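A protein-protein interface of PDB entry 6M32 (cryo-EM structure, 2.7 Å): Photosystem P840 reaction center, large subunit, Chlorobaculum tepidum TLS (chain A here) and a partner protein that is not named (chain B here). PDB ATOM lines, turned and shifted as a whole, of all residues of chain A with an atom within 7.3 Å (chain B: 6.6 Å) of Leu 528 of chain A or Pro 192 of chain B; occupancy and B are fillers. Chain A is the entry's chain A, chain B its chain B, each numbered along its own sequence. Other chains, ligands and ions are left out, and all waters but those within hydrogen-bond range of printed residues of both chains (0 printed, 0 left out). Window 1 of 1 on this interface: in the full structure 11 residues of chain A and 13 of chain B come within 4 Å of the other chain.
N of Lys 519 of chain A sits at hydrogen-bond distance from O of Pro 192 of chain B, at 3.1 Å.
NZ of Lys 519 of chain A lies close to O of Cys 191 of chain B.
The side-chain sulfur of Cys 191 of chain B lies close to the side-chain hydroxyl of Ser 193 of chain B (3.8 Å).
The backbone carbonyl oxygen of Trp 513 of chain A sits at hydrogen-bond distance from the backbone NH of Leu 518 of chain A.
The backbone NH (N) of Leu 528 of chain A is in hydrogen-bond range of the side-chain hydroxyl (OG1) of Thr 535 of chain A (2.9 Å).
The side-chain sulfur (SG) of Cys 143 of chain B lies close to the backbone NH (N) of Leu 145 of chain B, 3.7 Å away.
N of Gly 194 of chain B sits close to SG of Cys 191 of chain B.
The side-chain sulfur of Cys 191 of chain B sits close to the backbone NH of Ala 195 of chain B, 3.2 Å away.
Among the printed residues, pairs that only touch across the chains: Gly 517 of chain A with Pro 192 of chain B, Gly 517 of chain A with Ser 193 of chain B, Leu 518 of chain A with Pro 192 of chain B, Asn 521 of chain A with Glu 190 of chain B, Asn 521 of chain A with Cys 191 of chain B, Leu 528 of chain A with Cys 143 of chain B, Leu 528 of chain A with Pro 192 of chain B and Pro 530 of chain A with Phe 170 of chain B.
Of the printed residues of chain B, Lys 519 of chain A touches Cys 191 and Pro 192.
Of chain B, only Cys 143 and Pro 192 come within 4 Å of Leu 528 of chain A.
Leu 145 of chain B touches none of the printed residues of chain A.
Of chain A, only Gly 517 (3.7 Å), Leu 518 (3.1 Å), Lys 519 (3.1 Å) and Leu 528 (3.6 Å) come within 4 Å of Pro 192 of chain B.
Of the printed residues of chain A, Ser 193 of chain B touches Gly 517 (3.7 Å).
Gly 194 of chain B touches none of the printed residues of chain A.
The nearest residue of chain B that does not touch Leu 528 of chain A is Gly 142 of chain B (4.4 Å).
The nearest residue of chain A that does not touch Pro 192 of chain B is Asn 521 of chain A (4.3 Å).
The nearest printed residue of chain A that does not touch Cys 143 of chain B is Gly 529 of chain A (5.1 Å).
Of the 18 printed residues of chain A, 6 touch a printed residue of chain B.
Hydrophobic or aromatic side chains of chain A that line the printed part of chain B: Leu 528 and Pro 530.
Of the 12 printed residues of chain B, 6 touch a printed residue of chain A.
Hydrophobic or aromatic side chains of chain B within 4 Å of the printed part of chain A: Phe 170 and Pro 192.
Along chain B the printed residues that touch a printed residue of chain A span positions 143 to 193.
Among the printed residues, no Asp or Glu carboxylate lies within 4 Å of a Lys or Arg side-chain nitrogen of the other chain.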
ATOM      1  N   TRP A 513      11.780   2.209 -12.221  1.00  0.00           N
ATOM      2  CA  TRP A 513      11.578   0.878 -11.665  1.00  0.00           C
ATOM      3  C   TRP A 513      10.721   0.022 -12.584  1.00  0.00           C
ATOM      4  O   TRP A 513      10.930  -1.192 -12.672  1.00  0.00           O
ATOM      5  CB  TRP A 513      10.965   0.998 -10.273  1.00  0.00           C
ATOM      6  CG  TRP A 513      11.930   1.617  -9.318  1.00  0.00           C
ATOM      7  CD1 TRP A 513      11.981   2.927  -8.955  1.00  0.00           C
ATOM      8  CD2 TRP A 513      12.992   0.966  -8.614  1.00  0.00           C
ATOM      9  NE1 TRP A 513      13.006   3.137  -8.071  1.00  0.00           N
ATOM     10  CE2 TRP A 513      13.642   1.946  -7.842  1.00  0.00           C
ATOM     11  CE3 TRP A 513      13.452  -0.347  -8.555  1.00  0.00           C
ATOM     12  CZ2 TRP A 513      14.729   1.655  -7.026  1.00  0.00           C
ATOM     13  CZ3 TRP A 513      14.535  -0.635  -7.743  1.00  0.00           C
ATOM     14  CH2 TRP A 513      15.159   0.361  -6.989  1.00  0.00           C
ATOM     15  N   GLY A 517      12.524  -4.496 -14.564  1.00  0.00           N
ATOM     16  CA  GLY A 517      11.484  -5.299 -13.953  1.00  0.00           C
ATOM     17  C   GLY A 517      11.585  -5.320 -12.441  1.00  0.00           C
ATOM     18  O   GLY A 517      12.306  -6.159 -11.892  1.00  0.00           O
ATOM     19  N   LEU A 518      10.847  -4.453 -11.750  1.00  0.00           N
ATOM     20  CA  LEU A 518      11.056  -4.302 -10.316  1.00  0.00           C
ATOM     21  C   LEU A 518       9.781  -3.821  -9.629  1.00  0.00           C
ATOM     22  O   LEU A 518       8.838  -3.363 -10.279  1.00  0.00           O
ATOM     23  CB  LEU A 518      12.221  -3.344 -10.027  1.00  0.00           C
ATOM     24  CG  LEU A 518      13.610  -3.941 -10.283  1.00  0.00           C
ATOM     25  CD1 LEU A 518      14.693  -2.897 -10.341  1.00  0.00           C
ATOM     26  CD2 LEU A 518      13.932  -4.989  -9.240  1.00  0.00           C
ATOM     27  N   LYS A 519       9.779  -3.924  -8.299  1.00  0.00           N
ATOM     28  CA  LYS A 519       8.602  -3.702  -7.467  1.00  0.00           C
ATOM     29  C   LYS A 519       8.947  -2.732  -6.345  1.00  0.00           C
ATOM     30  O   LYS A 519      10.124  -2.486  -6.072  1.00  0.00           O
ATOM     31  CB  LYS A 519       8.123  -5.014  -6.839  1.00  0.00           C
ATOM     32  CG  LYS A 519       7.569  -6.061  -7.779  1.00  0.00           C
ATOM     33  CD  LYS A 519       7.154  -7.315  -7.042  1.00  0.00           C
ATOM     34  CE  LYS A 519       6.577  -8.366  -7.944  1.00  0.00           C
ATOM     35  NZ  LYS A 519       6.190  -9.613  -7.215  1.00  0.00           N
ATOM     36  N   LYS A 520       7.917  -2.166  -5.724  1.00  0.00           N
ATOM     37  CA  LYS A 520       7.984  -1.772  -4.327  1.00  0.00           C
ATOM     38  C   LYS A 520       6.799  -2.387  -3.596  1.00  0.00           C
ATOM     39  O   LYS A 520       5.657  -2.297  -4.055  1.00  0.00           O
ATOM     40  CB  LYS A 520       7.985  -0.253  -4.148  1.00  0.00           C
ATOM     41  CG  LYS A 520       9.059   0.481  -4.930  1.00  0.00           C
ATOM     42  CD  LYS A 520       8.571   1.841  -5.407  1.00  0.00           C
ATOM     43  CE  LYS A 520       9.650   2.567  -6.188  1.00  0.00           C
ATOM     44  NZ  LYS A 520       9.208   3.897  -6.672  1.00  0.00           N
ATOM     45  N   ASN A 521       7.074  -3.020  -2.460  1.00  0.00           N
ATOM     46  CA  ASN A 521       6.082  -3.876  -1.832  1.00  0.00           C
ATOM     47  C   ASN A 521       5.843  -3.618  -0.355  1.00  0.00           C
ATOM     48  O   ASN A 521       4.918  -4.214   0.207  1.00  0.00           O
ATOM     49  CB  ASN A 521       6.471  -5.350  -2.004  1.00  0.00           C
ATOM     50  CG  ASN A 521       6.490  -5.783  -3.450  1.00  0.00           C
ATOM     51  OD1 ASN A 521       5.707  -5.298  -4.265  1.00  0.00           O
ATOM     52  ND2 ASN A 521       7.377  -6.713  -3.776  1.00  0.00           N
ATOM     53  N   PHE A 525      10.901  -0.802   2.940  1.00  0.00           N
ATOM     54  CA  PHE A 525      12.119  -1.526   2.622  1.00  0.00           C
ATOM     55  C   PHE A 525      13.253  -0.532   2.391  1.00  0.00           C
ATOM     56  O   PHE A 525      13.065   0.480   1.708  1.00  0.00           O
ATOM     57  CB  PHE A 525      11.923  -2.417   1.394  1.00  0.00           C
ATOM     58  CG  PHE A 525      11.724  -1.661   0.118  1.00  0.00           C
ATOM     59  CD1 PHE A 525      10.509  -1.071  -0.169  1.00  0.00           C
ATOM     60  CD2 PHE A 525      12.751  -1.544  -0.798  1.00  0.00           C
ATOM     61  CE1 PHE A 525      10.324  -0.376  -1.341  1.00  0.00           C
ATOM     62  CE2 PHE A 525      12.571  -0.852  -1.971  1.00  0.00           C
ATOM     63  CZ  PHE A 525      11.357  -0.266  -2.243  1.00  0.00           C
ATOM     64  N   PRO A 526      14.425  -0.772   2.955  1.00  0.00           N
ATOM     65  CA  PRO A 526      15.470   0.255   2.941  1.00  0.00           C
ATOM     66  C   PRO A 526      16.147   0.406   1.591  1.00  0.00           C
ATOM     67  O   PRO A 526      16.491   1.521   1.189  1.00  0.00           O
ATOM     68  CB  PRO A 526      16.449  -0.244   4.005  1.00  0.00           C
ATOM     69  CG  PRO A 526      16.297  -1.715   3.985  1.00  0.00           C
ATOM     70  CD  PRO A 526      14.864  -2.004   3.632  1.00  0.00           C
ATOM     71  N   CYS A 527      16.337  -0.697   0.885  1.00  0.00           N
ATOM     72  CA  CYS A 527      17.089  -0.698  -0.364  1.00  0.00           C
ATOM     73  C   CYS A 527      16.832  -2.024  -1.066  1.00  0.00           C
ATOM     74  O   CYS A 527      15.982  -2.817  -0.642  1.00  0.00           O
ATOM     75  CB  CYS A 527      18.579  -0.488  -0.108  1.00  0.00           C
ATOM     76  SG  CYS A 527      19.364  -1.929   0.614  1.00  0.00           S
ATOM     77  N   LEU A 528      17.568  -2.265  -2.148  1.00  0.00           N
ATOM     78  CA  LEU A 528      17.532  -3.539  -2.842  1.00  0.00           C
ATOM     79  C   LEU A 528      18.912  -4.134  -3.062  1.00  0.00           C
ATOM     80  O   LEU A 528      19.011  -5.226  -3.630  1.00  0.00           O
ATOM     81  CB  LEU A 528      16.823  -3.399  -4.196  1.00  0.00           C
ATOM     82  CG  LEU A 528      15.298  -3.365  -4.145  1.00  0.00           C
ATOM     83  CD1 LEU A 528      14.725  -3.374  -5.547  1.00  0.00           C
ATOM     84  CD2 LEU A 528      14.772  -4.538  -3.340  1.00  0.00           C
ATOM     85  N   GLY A 529      19.972  -3.458  -2.636  1.00  0.00           N
ATOM     86  CA  GLY A 529      21.311  -3.954  -2.817  1.00  0.00           C
ATOM     87  C   GLY A 529      22.132  -3.065  -3.723  1.00  0.00           C
ATOM     88  O   GLY A 529      21.640  -2.078  -4.276  1.00  0.00           O
ATOM     89  N   PRO A 530      23.409  -3.405  -3.900  1.00  0.00           N
ATOM     90  CA  PRO A 530      24.302  -2.583  -4.720  1.00  0.00           C
ATOM     91  C   PRO A 530      24.093  -2.723  -6.217  1.00  0.00           C
ATOM     92  O   PRO A 530      24.913  -2.213  -6.985  1.00  0.00           O
ATOM     93  CB  PRO A 530      25.690  -3.104  -4.320  1.00  0.00           C
ATOM     94  CG  PRO A 530      25.456  -4.520  -3.968  1.00  0.00           C
ATOM     95  CD  PRO A 530      24.093  -4.582  -3.341  1.00  0.00           C
ATOM     96  N   VAL A 531      23.034  -3.402  -6.652  1.00  0.00           N
ATOM     97  CA  VAL A 531      22.809  -3.596  -8.076  1.00  0.00           C
ATOM     98  C   VAL A 531      22.505  -2.254  -8.729  1.00  0.00           C
ATOM     99  O   VAL A 531      21.877  -1.374  -8.124  1.00  0.00           O
ATOM    100  CB  VAL A 531      21.678  -4.615  -8.301  1.00  0.00           C
ATOM    101  CG1 VAL A 531      20.348  -4.069  -7.809  1.00  0.00           C
ATOM    102  CG2 VAL A 531      21.609  -5.033  -9.757  1.00  0.00           C
ATOM    103  N   GLY A 534      23.507   1.048  -6.807  1.00  0.00           N
ATOM    104  CA  GLY A 534      22.946   1.374  -5.511  1.00  0.00           C
ATOM    105  C   GLY A 534      21.484   1.750  -5.587  1.00  0.00           C
ATOM    106  O   GLY A 534      21.072   2.478  -6.491  1.00  0.00           O
ATOM    107  N   THR A 535      20.689   1.259  -4.642  1.00  0.00           N
ATOM    108  CA  THR A 535      19.244   1.452  -4.638  1.00  0.00           C
ATOM    109  C   THR A 535      18.763   1.890  -3.266  1.00  0.00           C
ATOM    110  O   THR A 535      17.811   1.335  -2.718  1.00  0.00           O
ATOM    111  CB  THR A 535      18.522   0.179  -5.067  1.00  0.00           C
ATOM    112  OG1 THR A 535      18.957  -0.911  -4.246  1.00  0.00           O
ATOM    113  CG2 THR A 535      18.810  -0.138  -6.524  1.00  0.00           C
ATOM    114  N   CYS A 536      19.413   2.892  -2.689  1.00  0.00           N
ATOM    115  CA  CYS A 536      19.132   3.331  -1.330  1.00  0.00           C
ATOM    116  C   CYS A 536      17.994   4.342  -1.328  1.00  0.00           C
ATOM    117  O   CYS A 536      17.906   5.188  -2.223  1.00  0.00           O
ATOM    118  CB  CYS A 536      20.381   3.961  -0.714  1.00  0.00           C
ATOM    119  SG  CYS A 536      21.778   2.858  -0.493  1.00  0.00           S
ATOM    120  N   GLY A 537      17.122   4.249  -0.326  1.00  0.00           N
ATOM    121  CA  GLY A 537      16.159   5.298  -0.061  1.00  0.00           C
ATOM    122  C   GLY A 537      15.132   5.543  -1.139  1.00  0.00           C
ATOM    123  O   GLY A 537      14.754   6.698  -1.370  1.00  0.00           O
ATOM    124  N   VAL A 538      14.672   4.494  -1.815  1.00  0.00           N
ATOM    125  CA  VAL A 538      13.638   4.617  -2.837  1.00  0.00           C
ATOM    126  C   VAL A 538      12.229   4.419  -2.293  1.00  0.00           C
ATOM    127  O   VAL A 538      11.274   4.957  -2.877  1.00  0.00           O
ATOM    128  CB  VAL A 538      13.926   3.651  -4.006  1.00  0.00           C
ATOM    129  CG1 VAL A 538      15.228   4.040  -4.693  1.00  0.00           C
ATOM    130  CG2 VAL A 538      14.061   2.215  -3.493  1.00  0.00           C
ATOM    131  N   VAL B 141      18.032 -10.212  -8.348  1.00  0.00           N
ATOM    132  CA  VAL B 141      18.912  -9.072  -8.134  1.00  0.00           C
ATOM    133  C   VAL B 141      19.713  -9.185  -6.849  1.00  0.00           C
ATOM    134  O   VAL B 141      20.591  -8.344  -6.610  1.00  0.00           O
ATOM    135  CB  VAL B 141      18.132  -7.740  -8.153  1.00  0.00           C
ATOM    136  CG1 VAL B 141      17.577  -7.478  -9.538  1.00  0.00           C
ATOM    137  CG2 VAL B 141      17.024  -7.760  -7.127  1.00  0.00           C
ATOM    138  N   GLY B 142      19.451 -10.189  -6.020  1.00  0.00           N
ATOM    139  CA  GLY B 142      20.251 -10.410  -4.832  1.00  0.00           C
ATOM    140  C   GLY B 142      19.874  -9.572  -3.632  1.00  0.00           C
ATOM    141  O   GLY B 142      20.698  -9.387  -2.730  1.00  0.00           O
ATOM    142  N   CYS B 143      18.640  -9.067  -3.583  1.00  0.00           N
ATOM    143  CA  CYS B 143      18.233  -8.257  -2.441  1.00  0.00           C
ATOM    144  C   CYS B 143      18.276  -9.051  -1.142  1.00  0.00           C
ATOM    145  O   CYS B 143      18.478  -8.471  -0.072  1.00  0.00           O
ATOM    146  CB  CYS B 143      16.838  -7.679  -2.674  1.00  0.00           C
ATOM    147  SG  CYS B 143      15.513  -8.889  -2.696  1.00  0.00           S
ATOM    148  N   GLY B 144      18.089 -10.369  -1.210  1.00  0.00           N
ATOM    149  CA  GLY B 144      18.223 -11.219  -0.049  1.00  0.00           C
ATOM    150  C   GLY B 144      17.009 -11.305   0.845  1.00  0.00           C
ATOM    151  O   GLY B 144      17.052 -12.030   1.846  1.00  0.00           O
ATOM    152  N   LEU B 145      15.927 -10.590   0.529  1.00  0.00           N
ATOM    153  CA  LEU B 145      14.717 -10.688   1.336  1.00  0.00           C
ATOM    154  C   LEU B 145      14.154 -12.100   1.352  1.00  0.00           C
ATOM    155  O   LEU B 145      13.549 -12.503   2.350  1.00  0.00           O
ATOM    156  CB  LEU B 145      13.661  -9.710   0.825  1.00  0.00           C
ATOM    157  CG  LEU B 145      14.145  -8.292   0.529  1.00  0.00           C
ATOM    158  CD1 LEU B 145      13.088  -7.516  -0.225  1.00  0.00           C
ATOM    159  CD2 LEU B 145      14.514  -7.572   1.812  1.00  0.00           C
ATOM    160  N   PHE B 170      25.695 -11.043  -7.787  1.00  0.00           N
ATOM    161  CA  PHE B 170      25.607 -11.838  -6.563  1.00  0.00           C
ATOM    162  C   PHE B 170      24.234 -12.473  -6.427  1.00  0.00           C
ATOM    163  O   PHE B 170      23.632 -12.473  -5.351  1.00  0.00           O
ATOM    164  CB  PHE B 170      25.947 -11.010  -5.326  1.00  0.00           C
ATOM    165  CG  PHE B 170      25.044  -9.837  -5.105  1.00  0.00           C
ATOM    166  CD1 PHE B 170      25.043  -8.768  -5.981  1.00  0.00           C
ATOM    167  CD2 PHE B 170      24.226  -9.786  -3.997  1.00  0.00           C
ATOM    168  CE1 PHE B 170      24.221  -7.688  -5.774  1.00  0.00           C
ATOM    169  CE2 PHE B 170      23.406  -8.708  -3.783  1.00  0.00           C
ATOM    170  CZ  PHE B 170      23.401  -7.658  -4.673  1.00  0.00           C
ATOM    171  N   GLU B 190       7.594 -10.616  -1.154  1.00  0.00           N
ATOM    172  CA  GLU B 190       8.742  -9.731  -1.000  1.00  0.00           C
ATOM    173  C   GLU B 190       9.594  -9.603  -2.252  1.00  0.00           C
ATOM    174  O   GLU B 190      10.264  -8.584  -2.423  1.00  0.00           O
ATOM    175  CB  GLU B 190       9.635 -10.200   0.154  1.00  0.00           C
ATOM    176  CG  GLU B 190      10.387 -11.498  -0.091  1.00  0.00           C
ATOM    177  CD  GLU B 190       9.582 -12.734   0.223  1.00  0.00           C
ATOM    178  OE1 GLU B 190       8.345 -12.635   0.346  1.00  0.00           O
ATOM    179  OE2 GLU B 190      10.202 -13.805   0.371  1.00  0.00           O
ATOM    180  N   CYS B 191       9.604 -10.603  -3.122  1.00  0.00           N
ATOM    181  CA  CYS B 191      10.491 -10.573  -4.275  1.00  0.00           C
ATOM    182  C   CYS B 191      10.095  -9.441  -5.212  1.00  0.00           C
ATOM    183  O   CYS B 191       8.933  -9.373  -5.634  1.00  0.00           O
ATOM    184  CB  CYS B 191      10.464 -11.903  -5.018  1.00  0.00           C
ATOM    185  SG  CYS B 191      11.759 -12.073  -6.264  1.00  0.00           S
ATOM    186  N   PRO B 192      11.011  -8.533  -5.553  1.00  0.00           N
ATOM    187  CA  PRO B 192      10.664  -7.423  -6.441  1.00  0.00           C
ATOM    188  C   PRO B 192      10.905  -7.683  -7.919  1.00  0.00           C
ATOM    189  O   PRO B 192      10.431  -6.897  -8.746  1.00  0.00           O
ATOM    190  CB  PRO B 192      11.568  -6.285  -5.931  1.00  0.00           C
ATOM    191  CG  PRO B 192      12.577  -6.935  -4.998  1.00  0.00           C
ATOM    192  CD  PRO B 192      12.380  -8.410  -5.039  1.00  0.00           C
ATOM    193  N   SER B 193      11.615  -8.747  -8.277  1.00  0.00           N
ATOM    194  CA  SER B 193      11.875  -9.055  -9.675  1.00  0.00           C
ATOM    195  C   SER B 193      11.012 -10.186 -10.214  1.00  0.00           C
ATOM    196  O   SER B 193      11.136 -10.524 -11.394  1.00  0.00           O
ATOM    197  CB  SER B 193      13.346  -9.420  -9.865  1.00  0.00           C
ATOM    198  OG  SER B 193      13.643 -10.641  -9.215  1.00  0.00           O
ATOM    199  N   GLY B 194      10.149 -10.772  -9.393  1.00  0.00           N
ATOM    200  CA  GLY B 194       9.437 -11.958  -9.818  1.00  0.00           C
ATOM    201  C   GLY B 194      10.337 -13.149 -10.051  1.00  0.00           C
ATOM    202  O   GLY B 194      10.141 -13.885 -11.021  1.00  0.00           O
ATOM    203  N   ALA B 195      11.325 -13.356  -9.184  1.00  0.00           N
ATOM    204  CA  ALA B 195      12.252 -14.468  -9.332  1.00  0.00           C
ATOM    205  C   ALA B 195      11.807 -15.716  -8.586  1.00  0.00           C
ATOM    206  O   ALA B 195      12.193 -16.823  -8.972  1.00  0.00           O
ATOM    207  CB  ALA B 195      13.646 -14.056  -8.857  1.00  0.00           C
